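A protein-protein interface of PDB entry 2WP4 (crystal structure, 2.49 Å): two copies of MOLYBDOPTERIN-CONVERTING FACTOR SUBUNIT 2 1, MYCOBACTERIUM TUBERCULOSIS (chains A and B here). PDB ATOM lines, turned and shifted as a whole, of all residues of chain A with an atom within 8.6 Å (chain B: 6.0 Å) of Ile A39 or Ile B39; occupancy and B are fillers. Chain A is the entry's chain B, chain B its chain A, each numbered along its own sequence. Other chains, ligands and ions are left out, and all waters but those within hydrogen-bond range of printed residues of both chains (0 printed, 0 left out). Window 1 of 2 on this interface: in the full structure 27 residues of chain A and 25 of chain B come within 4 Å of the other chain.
The backbone carbonyl oxygen (O) of Ile A37 is in hydrogen-bond range of the backbone NH (N) of Val B41 (2.8 Å). O of Ile B37 is in hydrogen-bond range of N of Val A41 (2.8 Å). The backbone carbonyl oxygen of Ile A39 lies within hydrogen-bond range of the backbone NH of Ile B39 (2.8 Å).
The backbone NH (N) of Val B38 is in hydrogen-bond range of the backbone carbonyl oxygen (O) of Ala B105 (2.8 Å). N of Phe B40 is in hydrogen-bond range of O of Ile B103, at 2.7 Å. The backbone carbonyl oxygen (O) of Leu A26 sits at hydrogen-bond distance from the side-chain hydroxyl (OG) of Ser A30 (2.8 Å). The backbone NH (N) of Ile A103 is in hydrogen-bond range of the backbone carbonyl oxygen (O) of Phe A40, at 2.7 Å. The backbone NH of Val A38 sits at hydrogen-bond distance from the backbone carbonyl oxygen of Ala A105, 2.7 Å away.
Among the printed residues, pairs that only touch across the chains: Ile A39 with Val B38, Phe A40 with Ile B37, Ile A37 with Phe B40, Val A38 with Ile B39, Ile A39 with Ile B37, Ile A37 with Ile B39, Phe A114 with Phe B40, Gly A36 with Val B41, Val A38 with Val B38, Gly A36 with Phe B40, Val A22 with Val B22, Val A38 with Phe B40 and Leu A26 with Val B22.
Of chain A, only Ile A37, Val A38 and Ile A39 come within 4 Å of Ile B39. Printed residues of chain B within 4 Å of Ile A37: Ile B39, Phe B40 and Val B41. Of the printed residues of chain A, Ile B37 touches Ile A39 (3.5 Å), Phe A40 (3.3 Å) and Val A41 (2.8 Å). Leu B26 touches none of the printed residues of chain A. Ala A27 touches none of the printed residues of chain B. The nearest residue of chain B that does not touch Ile A39 is Val B41 (5.0 Å). The nearest printed residue of chain B that does not touch Val A22 is Leu B26 (4.3 Å).
Hydrophobic or aromatic side chains of chain B that line the printed part of chain A: Val B22, Ile B37, Val B38 and Phe B40. Among the printed residues, 16 pairs touch across the chains. Among the printed residues, no Asp or Glu carboxylate lies within 4 Å of a Lys or Arg side-chain nitrogen of the other chain.
Val B22 touches its own counterpart, Val A22. Ile A37 touches Ile B39, and with the chains exchanged Ile A39 touches Ile B37. Val A38 touches Phe B40, but with the chains exchanged Phe A40 does not touch Val B38 (4.1 Å). Ile A39 touches its own counterpart, Ile B39.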
ATOM      1  N   SER A  21      20.125  13.435 -24.784  1.00  0.00           N
ATOM      2  CA  SER A  21      19.071  14.078 -25.572  1.00  0.00           C
ATOM      3  C   SER A  21      17.721  14.026 -24.868  1.00  0.00           C
ATOM      4  O   SER A  21      17.210  12.946 -24.541  1.00  0.00           O
ATOM      5  CB  SER A  21      18.964  13.428 -26.955  1.00  0.00           C
ATOM      6  OG  SER A  21      17.725  13.752 -27.569  1.00  0.00           O
ATOM      7  N   VAL A  22      17.151  15.198 -24.642  1.00  0.00           N
ATOM      8  CA  VAL A  22      15.810  15.315 -24.092  1.00  0.00           C
ATOM      9  C   VAL A  22      14.767  14.765 -25.071  1.00  0.00           C
ATOM     10  O   VAL A  22      13.898  13.978 -24.684  1.00  0.00           O
ATOM     11  CB  VAL A  22      15.498  16.780 -23.701  1.00  0.00           C
ATOM     12  CG1 VAL A  22      13.998  17.003 -23.543  1.00  0.00           C
ATOM     13  CG2 VAL A  22      16.251  17.146 -22.411  1.00  0.00           C
ATOM     14  N   ASP A  23      14.877  15.173 -26.333  1.00  0.00           N
ATOM     15  CA  ASP A  23      13.962  14.726 -27.393  1.00  0.00           C
ATOM     16  C   ASP A  23      13.797  13.191 -27.432  1.00  0.00           C
ATOM     17  O   ASP A  23      12.674  12.689 -27.557  1.00  0.00           O
ATOM     18  CB  ASP A  23      14.420  15.250 -28.767  1.00  0.00           C
ATOM     19  CG  ASP A  23      14.309  16.782 -28.896  1.00  0.00           C
ATOM     20  OD1 ASP A  23      13.485  17.411 -28.184  1.00  0.00           O
ATOM     21  OD2 ASP A  23      15.051  17.362 -29.739  1.00  0.00           O
ATOM     22  N   GLU A  24      14.907  12.458 -27.312  1.00  0.00           N
ATOM     23  CA  GLU A  24      14.880  10.998 -27.416  1.00  0.00           C
ATOM     24  C   GLU A  24      14.134  10.390 -26.245  1.00  0.00           C
ATOM     25  O   GLU A  24      13.308   9.498 -26.413  1.00  0.00           O
ATOM     26  CB  GLU A  24      16.294  10.414 -27.516  1.00  0.00           C
ATOM     27  CG  GLU A  24      16.998  10.728 -28.846  1.00  0.00           C
ATOM     28  CD  GLU A  24      18.405  10.136 -28.943  1.00  0.00           C
ATOM     29  OE1 GLU A  24      19.105  10.436 -29.935  1.00  0.00           O
ATOM     30  OE2 GLU A  24      18.817   9.378 -28.035  1.00  0.00           O
ATOM     31  N   VAL A  25      14.425  10.898 -25.057  1.00  0.00           N
ATOM     32  CA  VAL A  25      13.754  10.469 -23.842  1.00  0.00           C
ATOM     33  C   VAL A  25      12.279  10.848 -23.898  1.00  0.00           C
ATOM     34  O   VAL A  25      11.420  10.044 -23.561  1.00  0.00           O
ATOM     35  CB  VAL A  25      14.467  11.035 -22.596  1.00  0.00           C
ATOM     36  CG1 VAL A  25      13.605  10.918 -21.351  1.00  0.00           C
ATOM     37  CG2 VAL A  25      15.796  10.315 -22.396  1.00  0.00           C
ATOM     38  N   LEU A  26      11.996  12.058 -24.367  1.00  0.00           N
ATOM     39  CA  LEU A  26      10.625  12.521 -24.556  1.00  0.00           C
ATOM     40  C   LEU A  26       9.838  11.590 -25.481  1.00  0.00           C
ATOM     41  O   LEU A  26       8.732  11.144 -25.129  1.00  0.00           O
ATOM     42  CB  LEU A  26      10.609  13.966 -25.078  1.00  0.00           C
ATOM     43  CG  LEU A  26       9.250  14.674 -25.170  1.00  0.00           C
ATOM     44  CD1 LEU A  26       8.574  14.754 -23.812  1.00  0.00           C
ATOM     45  CD2 LEU A  26       9.383  16.070 -25.767  1.00  0.00           C
ATOM     46  N   ALA A  27      10.410  11.289 -26.650  1.00  0.00           N
ATOM     47  CA  ALA A  27       9.793  10.357 -27.598  1.00  0.00           C
ATOM     48  C   ALA A  27       9.565   8.980 -26.963  1.00  0.00           C
ATOM     49  O   ALA A  27       8.509   8.384 -27.144  1.00  0.00           O
ATOM     50  CB  ALA A  27      10.627  10.240 -28.861  1.00  0.00           C
ATOM     51  N   ALA A  28      10.541   8.510 -26.188  1.00  0.00           N
ATOM     52  CA  ALA A  28      10.482   7.201 -25.539  1.00  0.00           C
ATOM     53  C   ALA A  28       9.285   6.999 -24.596  1.00  0.00           C
ATOM     54  O   ALA A  28       8.835   5.870 -24.410  1.00  0.00           O
ATOM     55  CB  ALA A  28      11.789   6.918 -24.802  1.00  0.00           C
ATOM     56  N   VAL A  29       8.785   8.077 -23.994  1.00  0.00           N
ATOM     57  CA  VAL A  29       7.647   7.976 -23.076  1.00  0.00           C
ATOM     58  C   VAL A  29       6.330   8.536 -23.633  1.00  0.00           C
ATOM     59  O   VAL A  29       5.311   8.551 -22.939  1.00  0.00           O
ATOM     60  CB  VAL A  29       7.951   8.599 -21.674  1.00  0.00           C
ATOM     61  CG1 VAL A  29       9.080   7.839 -20.996  1.00  0.00           C
ATOM     62  CG2 VAL A  29       8.242  10.103 -21.764  1.00  0.00           C
ATOM     63  N   SER A  30       6.351   8.982 -24.886  1.00  0.00           N
ATOM     64  CA  SER A  30       5.159   9.544 -25.514  1.00  0.00           C
ATOM     65  C   SER A  30       4.238   8.450 -26.008  1.00  0.00           C
ATOM     66  O   SER A  30       4.689   7.372 -26.368  1.00  0.00           O
ATOM     67  CB  SER A  30       5.536  10.470 -26.666  1.00  0.00           C
ATOM     68  OG  SER A  30       6.144  11.647 -26.167  1.00  0.00           O
ATOM     69  N   GLY A  36       0.333  13.415 -19.505  1.00  0.00           N
ATOM     70  CA  GLY A  36       1.266  14.195 -18.706  1.00  0.00           C
ATOM     71  C   GLY A  36       2.662  13.608 -18.789  1.00  0.00           C
ATOM     72  O   GLY A  36       2.854  12.415 -18.556  1.00  0.00           O
ATOM     73  N   ILE A  37       3.636  14.445 -19.131  1.00  0.00           N
ATOM     74  CA  ILE A  37       5.012  13.992 -19.259  1.00  0.00           C
ATOM     75  C   ILE A  37       5.943  14.888 -18.459  1.00  0.00           C
ATOM     76  O   ILE A  37       5.906  16.112 -18.594  1.00  0.00           O
ATOM     77  CB  ILE A  37       5.485  13.955 -20.734  1.00  0.00           C
ATOM     78  CG1 ILE A  37       4.567  13.063 -21.581  1.00  0.00           C
ATOM     79  CG2 ILE A  37       6.946  13.498 -20.809  1.00  0.00           C
ATOM     80  CD1 ILE A  37       4.922  13.042 -23.047  1.00  0.00           C
ATOM     81  N   VAL A  38       6.784  14.269 -17.637  1.00  0.00           N
ATOM     82  CA  VAL A  38       7.773  14.998 -16.854  1.00  0.00           C
ATOM     83  C   VAL A  38       9.190  14.547 -17.198  1.00  0.00           C
ATOM     84  O   VAL A  38       9.501  13.351 -17.178  1.00  0.00           O
ATOM     85  CB  VAL A  38       7.509  14.847 -15.346  1.00  0.00           C
ATOM     86  CG1 VAL A  38       8.617  15.506 -14.535  1.00  0.00           C
ATOM     87  CG2 VAL A  38       6.134  15.436 -14.987  1.00  0.00           C
ATOM     88  N   ILE A  39      10.036  15.518 -17.523  1.00  0.00           N
ATOM     89  CA  ILE A  39      11.446  15.273 -17.793  1.00  0.00           C
ATOM     90  C   ILE A  39      12.296  15.951 -16.730  1.00  0.00           C
ATOM     91  O   ILE A  39      12.130  17.142 -16.473  1.00  0.00           O
ATOM     92  CB  ILE A  39      11.845  15.773 -19.198  1.00  0.00           C
ATOM     93  CG1 ILE A  39      11.114  14.937 -20.254  1.00  0.00           C
ATOM     94  CG2 ILE A  39      13.354  15.679 -19.405  1.00  0.00           C
ATOM     95  CD1 ILE A  39      11.113  15.558 -21.612  1.00  0.00           C
ATOM     96  N   PHE A  40      13.165  15.169 -16.086  1.00  0.00           N
ATOM     97  CA  PHE A  40      14.218  15.716 -15.249  1.00  0.00           C
ATOM     98  C   PHE A  40      15.586  15.631 -15.937  1.00  0.00           C
ATOM     99  O   PHE A  40      15.963  14.581 -16.471  1.00  0.00           O
ATOM    100  CB  PHE A  40      14.282  15.041 -13.875  1.00  0.00           C
ATOM    101  CG  PHE A  40      15.479  15.472 -13.065  1.00  0.00           C
ATOM    102  CD1 PHE A  40      15.533  16.749 -12.506  1.00  0.00           C
ATOM    103  CD2 PHE A  40      16.575  14.630 -12.904  1.00  0.00           C
ATOM    104  CE1 PHE A  40      16.644  17.168 -11.790  1.00  0.00           C
ATOM    105  CE2 PHE A  40      17.696  15.054 -12.176  1.00  0.00           C
ATOM    106  CZ  PHE A  40      17.725  16.312 -11.621  1.00  0.00           C
ATOM    107  N   VAL A  41      16.319  16.741 -15.905  1.00  0.00           N
ATOM    108  CA  VAL A  41      17.687  16.803 -16.414  1.00  0.00           C
ATOM    109  C   VAL A  41      18.579  17.207 -15.255  1.00  0.00           C
ATOM    110  O   VAL A  41      18.395  18.288 -14.672  1.00  0.00           O
ATOM    111  CB  VAL A  41      17.847  17.871 -17.537  1.00  0.00           C
ATOM    112  CG1 VAL A  41      19.259  17.871 -18.099  1.00  0.00           C
ATOM    113  CG2 VAL A  41      16.813  17.673 -18.648  1.00  0.00           C
ATOM    114  N   GLY A  42      19.540  16.341 -14.921  1.00  0.00           N
ATOM    115  CA  GLY A  42      20.525  16.624 -13.879  1.00  0.00           C
ATOM    116  C   GLY A  42      21.809  17.091 -14.523  1.00  0.00           C
ATOM    117  O   GLY A  42      22.451  16.330 -15.251  1.00  0.00           O
ATOM    118  N   ALA A  86      11.772   6.287 -18.438  1.00  0.00           N
ATOM    119  CA  ALA A  86      12.935   6.153 -19.318  1.00  0.00           C
ATOM    120  C   ALA A  86      14.127   6.868 -18.707  1.00  0.00           C
ATOM    121  O   ALA A  86      13.986   7.970 -18.167  1.00  0.00           O
ATOM    122  CB  ALA A  86      12.630   6.733 -20.698  1.00  0.00           C
ATOM    123  N   VAL A 101      22.353  13.163 -16.418  1.00  0.00           N
ATOM    124  CA  VAL A 101      21.204  12.283 -16.447  1.00  0.00           C
ATOM    125  C   VAL A 101      20.010  13.002 -17.079  1.00  0.00           C
ATOM    126  O   VAL A 101      19.808  14.203 -16.872  1.00  0.00           O
ATOM    127  CB  VAL A 101      20.865  11.728 -15.020  1.00  0.00           C
ATOM    128  CG1 VAL A 101      20.513  12.861 -14.034  1.00  0.00           C
ATOM    129  CG2 VAL A 101      19.752  10.687 -15.083  1.00  0.00           C
ATOM    130  N   VAL A 102      19.255  12.266 -17.891  1.00  0.00           N
ATOM    131  CA  VAL A 102      17.951  12.704 -18.361  1.00  0.00           C
ATOM    132  C   VAL A 102      16.941  11.610 -18.019  1.00  0.00           C
ATOM    133  O   VAL A 102      17.107  10.447 -18.404  1.00  0.00           O
ATOM    134  CB  VAL A 102      17.940  13.008 -19.882  1.00  0.00           C
ATOM    135  CG1 VAL A 102      16.508  13.303 -20.372  1.00  0.00           C
ATOM    136  CG2 VAL A 102      18.876  14.186 -20.217  1.00  0.00           C
ATOM    137  N   ILE A 103      15.908  11.983 -17.272  1.00  0.00           N
ATOM    138  CA  ILE A 103      14.854  11.047 -16.913  1.00  0.00           C
ATOM    139  C   ILE A 103      13.528  11.519 -17.483  1.00  0.00           C
ATOM    140  O   ILE A 103      13.222  12.715 -17.453  1.00  0.00           O
ATOM    141  CB  ILE A 103      14.755  10.868 -15.389  1.00  0.00           C
ATOM    142  CG1 ILE A 103      15.928  10.017 -14.900  1.00  0.00           C
ATOM    143  CG2 ILE A 103      13.400  10.225 -14.978  1.00  0.00           C
ATOM    144  CD1 ILE A 103      16.091  10.023 -13.398  1.00  0.00           C
ATOM    145  N   GLY A 104      12.756  10.575 -18.015  1.00  0.00           N
ATOM    146  CA  GLY A 104      11.410  10.859 -18.481  1.00  0.00           C
ATOM    147  C   GLY A 104      10.403   9.940 -17.816  1.00  0.00           C
ATOM    148  O   GLY A 104      10.647   8.745 -17.656  1.00  0.00           O
ATOM    149  N   ALA A 105       9.267  10.508 -17.428  1.00  0.00           N
ATOM    150  CA  ALA A 105       8.142   9.729 -16.922  1.00  0.00           C
ATOM    151  C   ALA A 105       6.851  10.298 -17.497  1.00  0.00           C
ATOM    152  O   ALA A 105       6.662  11.529 -17.536  1.00  0.00           O
ATOM    153  CB  ALA A 105       8.112   9.746 -15.403  1.00  0.00           C
ATOM    154  N   SER A 106       5.978   9.406 -17.954  1.00  0.00           N
ATOM    155  CA  SER A 106       4.691   9.795 -18.478  1.00  0.00           C
ATOM    156  C   SER A 106       3.597   8.942 -17.861  1.00  0.00           C
ATOM    157  O   SER A 106       3.872   7.901 -17.251  1.00  0.00           O
ATOM    158  CB  SER A 106       4.667   9.673 -19.999  1.00  0.00           C
ATOM    159  OG  SER A 106       4.746   8.319 -20.406  1.00  0.00           O
ATOM    160  N   ALA A 113       2.941  11.226 -13.241  1.00  0.00           N
ATOM    161  CA  ALA A 113       4.142  11.512 -14.011  1.00  0.00           C
ATOM    162  C   ALA A 113       5.180  12.188 -13.137  1.00  0.00           C
ATOM    163  O   ALA A 113       6.350  11.833 -13.197  1.00  0.00           O
ATOM    164  CB  ALA A 113       3.808  12.363 -15.238  1.00  0.00           C
ATOM    165  N   PHE A 114       4.744  13.150 -12.325  1.00  0.00           N
ATOM    166  CA  PHE A 114       5.618  13.814 -11.345  1.00  0.00           C
ATOM    167  C   PHE A 114       6.131  12.829 -10.296  1.00  0.00           C
ATOM    168  O   PHE A 114       7.323  12.815  -9.986  1.00  0.00           O
ATOM    169  CB  PHE A 114       4.890  14.974 -10.658  1.00  0.00           C
ATOM    170  CG  PHE A 114       4.878  16.250 -11.461  1.00  0.00           C
ATOM    171  CD1 PHE A 114       5.910  17.191 -11.318  1.00  0.00           C
ATOM    172  CD2 PHE A 114       3.835  16.525 -12.350  1.00  0.00           C
ATOM    173  CE1 PHE A 114       5.909  18.380 -12.053  1.00  0.00           C
ATOM    174  CE2 PHE A 114       3.818  17.714 -13.091  1.00  0.00           C
ATOM    175  CZ  PHE A 114       4.863  18.648 -12.938  1.00  0.00           C
ATOM    176  N   ALA A 117       8.721  10.449 -11.978  1.00  0.00           N
ATOM    177  CA  ALA A 117       9.977  11.146 -12.268  1.00  0.00           C
ATOM    178  C   ALA A 117      10.776  11.362 -10.987  1.00  0.00           C
ATOM    179  O   ALA A 117      11.981  11.102 -10.960  1.00  0.00           O
ATOM    180  CB  ALA A 117       9.717  12.472 -12.967  1.00  0.00           C
ATOM    181  N   ARG A 118      10.100  11.822  -9.933  1.00  0.00           N
ATOM    182  CA  ARG A 118      10.758  12.081  -8.655  1.00  0.00           C
ATOM    183  C   ARG A 118      11.273  10.799  -8.024  1.00  0.00           C
ATOM    184  O   ARG A 118      12.422  10.741  -7.598  1.00  0.00           O
ATOM    185  CB  ARG A 118       9.841  12.827  -7.682  1.00  0.00           C
ATOM    186  CG  ARG A 118      10.565  13.340  -6.439  1.00  0.00           C
ATOM    187  CD  ARG A 118      11.667  14.340  -6.801  1.00  0.00           C
ATOM    188  NE  ARG A 118      12.494  14.739  -5.660  1.00  0.00           N
ATOM    189  CZ  ARG A 118      12.214  15.747  -4.833  1.00  0.00           C
ATOM    190  NH1 ARG A 118      11.111  16.467  -4.996  1.00  0.00           N
ATOM    191  NH2 ARG A 118      13.041  16.037  -3.834  1.00  0.00           N
ATOM    192  N   VAL B  22      10.206  22.482 -27.071  1.00  0.00           N
ATOM    193  CA  VAL B  22      10.847  22.015 -25.850  1.00  0.00           C
ATOM    194  C   VAL B  22      12.257  22.587 -25.761  1.00  0.00           C
ATOM    195  O   VAL B  22      12.680  23.010 -24.686  1.00  0.00           O
ATOM    196  CB  VAL B  22      10.854  20.469 -25.755  1.00  0.00           C
ATOM    197  CG1 VAL B  22      11.890  19.984 -24.730  1.00  0.00           C
ATOM    198  CG2 VAL B  22       9.459  19.952 -25.396  1.00  0.00           C
ATOM    199  N   VAL B  25      12.070  26.234 -24.410  1.00  0.00           N
ATOM    200  CA  VAL B  25      11.756  26.256 -22.979  1.00  0.00           C
ATOM    201  C   VAL B  25      12.971  25.790 -22.174  1.00  0.00           C
ATOM    202  O   VAL B  25      13.313  26.377 -21.150  1.00  0.00           O
ATOM    203  CB  VAL B  25      10.505  25.391 -22.666  1.00  0.00           C
ATOM    204  CG1 VAL B  25      10.463  24.971 -21.205  1.00  0.00           C
ATOM    205  CG2 VAL B  25       9.227  26.142 -23.049  1.00  0.00           C
ATOM    206  N   LEU B  26      13.636  24.751 -22.671  1.00  0.00           N
ATOM    207  CA  LEU B  26      14.823  24.212 -22.025  1.00  0.00           C
ATOM    208  C   LEU B  26      15.970  25.223 -22.001  1.00  0.00           C
ATOM    209  O   LEU B  26      16.638  25.384 -20.977  1.00  0.00           O
ATOM    210  CB  LEU B  26      15.253  22.915 -22.720  1.00  0.00           C
ATOM    211  CG  LEU B  26      16.597  22.298 -22.353  1.00  0.00           C
ATOM    212  CD1 LEU B  26      16.546  21.691 -20.955  1.00  0.00           C
ATOM    213  CD2 LEU B  26      16.979  21.259 -23.392  1.00  0.00           C
ATOM    214  N   VAL B  29      15.793  28.288 -19.497  1.00  0.00           N
ATOM    215  CA  VAL B  29      15.784  27.885 -18.115  1.00  0.00           C
ATOM    216  C   VAL B  29      17.163  27.298 -17.746  1.00  0.00           C
ATOM    217  O   VAL B  29      17.441  27.000 -16.587  1.00  0.00           O
ATOM    218  CB  VAL B  29      14.551  26.932 -17.916  1.00  0.00           C
ATOM    219  CG1 VAL B  29      14.905  25.578 -17.354  1.00  0.00           C
ATOM    220  CG2 VAL B  29      13.412  27.635 -17.155  1.00  0.00           C
ATOM    221  N   ILE B  37      16.773  20.594 -13.694  1.00  0.00           N
ATOM    222  CA  ILE B  37      15.769  21.100 -14.624  1.00  0.00           C
ATOM    223  C   ILE B  37      14.621  20.103 -14.740  1.00  0.00           C
ATOM    224  O   ILE B  37      14.827  18.916 -15.058  1.00  0.00           O
ATOM    225  CB  ILE B  37      16.346  21.358 -16.039  1.00  0.00           C
ATOM    226  CG1 ILE B  37      17.539  22.331 -15.978  1.00  0.00           C
ATOM    227  CG2 ILE B  37      15.234  21.866 -16.998  1.00  0.00           C
ATOM    228  CD1 ILE B  37      18.233  22.537 -17.306  1.00  0.00           C
ATOM    229  N   VAL B  38      13.418  20.600 -14.457  1.00  0.00           N
ATOM    230  CA  VAL B  38      12.188  19.847 -14.650  1.00  0.00           C
ATOM    231  C   VAL B  38      11.368  20.475 -15.772  1.00  0.00           C
ATOM    232  O   VAL B  38      11.161  21.694 -15.812  1.00  0.00           O
ATOM    233  CB  VAL B  38      11.361  19.732 -13.344  1.00  0.00           C
ATOM    234  CG1 VAL B  38      10.072  18.924 -13.588  1.00  0.00           C
ATOM    235  CG2 VAL B  38      12.196  19.058 -12.252  1.00  0.00           C
ATOM    236  N   ILE B  39      10.927  19.630 -16.698  1.00  0.00           N
ATOM    237  CA  ILE B  39      10.125  20.067 -17.828  1.00  0.00           C
ATOM    238  C   ILE B  39       8.822  19.296 -17.817  1.00  0.00           C
ATOM    239  O   ILE B  39       8.818  18.060 -17.774  1.00  0.00           O
ATOM    240  CB  ILE B  39      10.867  19.838 -19.158  1.00  0.00           C
ATOM    241  CG1 ILE B  39      11.991  20.861 -19.319  1.00  0.00           C
ATOM    242  CG2 ILE B  39       9.909  19.939 -20.368  1.00  0.00           C
ATOM    243  CD1 ILE B  39      13.021  20.418 -20.301  1.00  0.00           C
ATOM    244  N   PHE B  40       7.710  20.019 -17.822  1.00  0.00           N
ATOM    245  CA  PHE B  40       6.421  19.361 -17.944  1.00  0.00           C
ATOM    246  C   PHE B  40       5.815  19.591 -19.325  1.00  0.00           C
ATOM    247  O   PHE B  40       5.727  20.723 -19.801  1.00  0.00           O
ATOM    248  CB  PHE B  40       5.429  19.783 -16.855  1.00  0.00           C
ATOM    249  CG  PHE B  40       4.048  19.241 -17.092  1.00  0.00           C
ATOM    250  CD1 PHE B  40       3.728  17.935 -16.724  1.00  0.00           C
ATOM    251  CD2 PHE B  40       3.080  20.010 -17.747  1.00  0.00           C
ATOM    252  CE1 PHE B  40       2.451  17.406 -16.976  1.00  0.00           C
ATOM    253  CE2 PHE B  40       1.802  19.488 -17.997  1.00  0.00           C
ATOM    254  CZ  PHE B  40       1.492  18.183 -17.607  1.00  0.00           C
ATOM    255  N   VAL B  41       5.391  18.503 -19.952  1.00  0.00           N
ATOM    256  CA  VAL B  41       4.730  18.556 -21.246  1.00  0.00           C
ATOM    257  C   VAL B  41       3.320  17.997 -21.104  1.00  0.00           C
ATOM    258  O   VAL B  41       3.136  16.847 -20.679  1.00  0.00           O
ATOM    259  CB  VAL B  41       5.531  17.777 -22.323  1.00  0.00           C
ATOM    260  CG1 VAL B  41       4.870  17.904 -23.701  1.00  0.00           C
ATOM    261  CG2 VAL B  41       6.967  18.295 -22.370  1.00  0.00           C
ATOM    262  N   VAL B 102       3.948  23.491 -22.426  1.00  0.00           N
ATOM    263  CA  VAL B 102       5.302  23.080 -22.047  1.00  0.00           C
ATOM    264  C   VAL B 102       5.811  24.051 -20.988  1.00  0.00           C
ATOM    265  O   VAL B 102       5.825  25.275 -21.198  1.00  0.00           O
ATOM    266  CB  VAL B 102       6.278  23.064 -23.249  1.00  0.00           C
ATOM    267  CG1 VAL B 102       7.689  22.712 -22.780  1.00  0.00           C
ATOM    268  CG2 VAL B 102       5.798  22.078 -24.359  1.00  0.00           C
ATOM    269  N   ILE B 103       6.211  23.503 -19.844  1.00  0.00           N
ATOM    270  CA  ILE B 103       6.686  24.289 -18.715  1.00  0.00           C
ATOM    271  C   ILE B 103       8.089  23.812 -18.401  1.00  0.00           C
ATOM    272  O   ILE B 103       8.362  22.610 -18.445  1.00  0.00           O
ATOM    273  CB  ILE B 103       5.781  24.078 -17.474  1.00  0.00           C
ATOM    274  CG1 ILE B 103       4.465  24.818 -17.647  1.00  0.00           C
ATOM    275  CG2 ILE B 103       6.474  24.527 -16.180  1.00  0.00           C
ATOM    276  CD1 ILE B 103       3.366  24.318 -16.733  1.00  0.00           C
ATOM    277  N   GLY B 104       8.972  24.760 -18.102  1.00  0.00           N
ATOM    278  CA  GLY B 104      10.326  24.471 -17.662  1.00  0.00           C
ATOM    279  C   GLY B 104      10.588  25.199 -16.357  1.00  0.00           C
ATOM    280  O   GLY B 104      10.209  26.365 -16.203  1.00  0.00           O
ATOM    281  N   ALA B 105      11.210  24.497 -15.411  1.00  0.00           N
ATOM    282  CA  ALA B 105      11.672  25.097 -14.167  1.00  0.00           C
ATOM    283  C   ALA B 105      13.039  24.534 -13.838  1.00  0.00           C
ATOM    284  O   ALA B 105      13.256  23.323 -13.941  1.00  0.00           O
ATOM    285  CB  ALA B 105      10.694  24.826 -13.024  1.00  0.00           C
ATOM    286  N   ALA B 117       8.076  23.605 -11.032  1.00  0.00           N
ATOM    287  CA  ALA B 117       7.353  23.029 -12.177  1.00  0.00           C
ATOM    288  C   ALA B 117       5.948  22.555 -11.798  1.00  0.00           C
ATOM    289  O   ALA B 117       5.003  22.798 -12.540  1.00  0.00           O
ATOM    290  CB  ALA B 117       8.141  21.887 -12.803  1.00  0.00           C
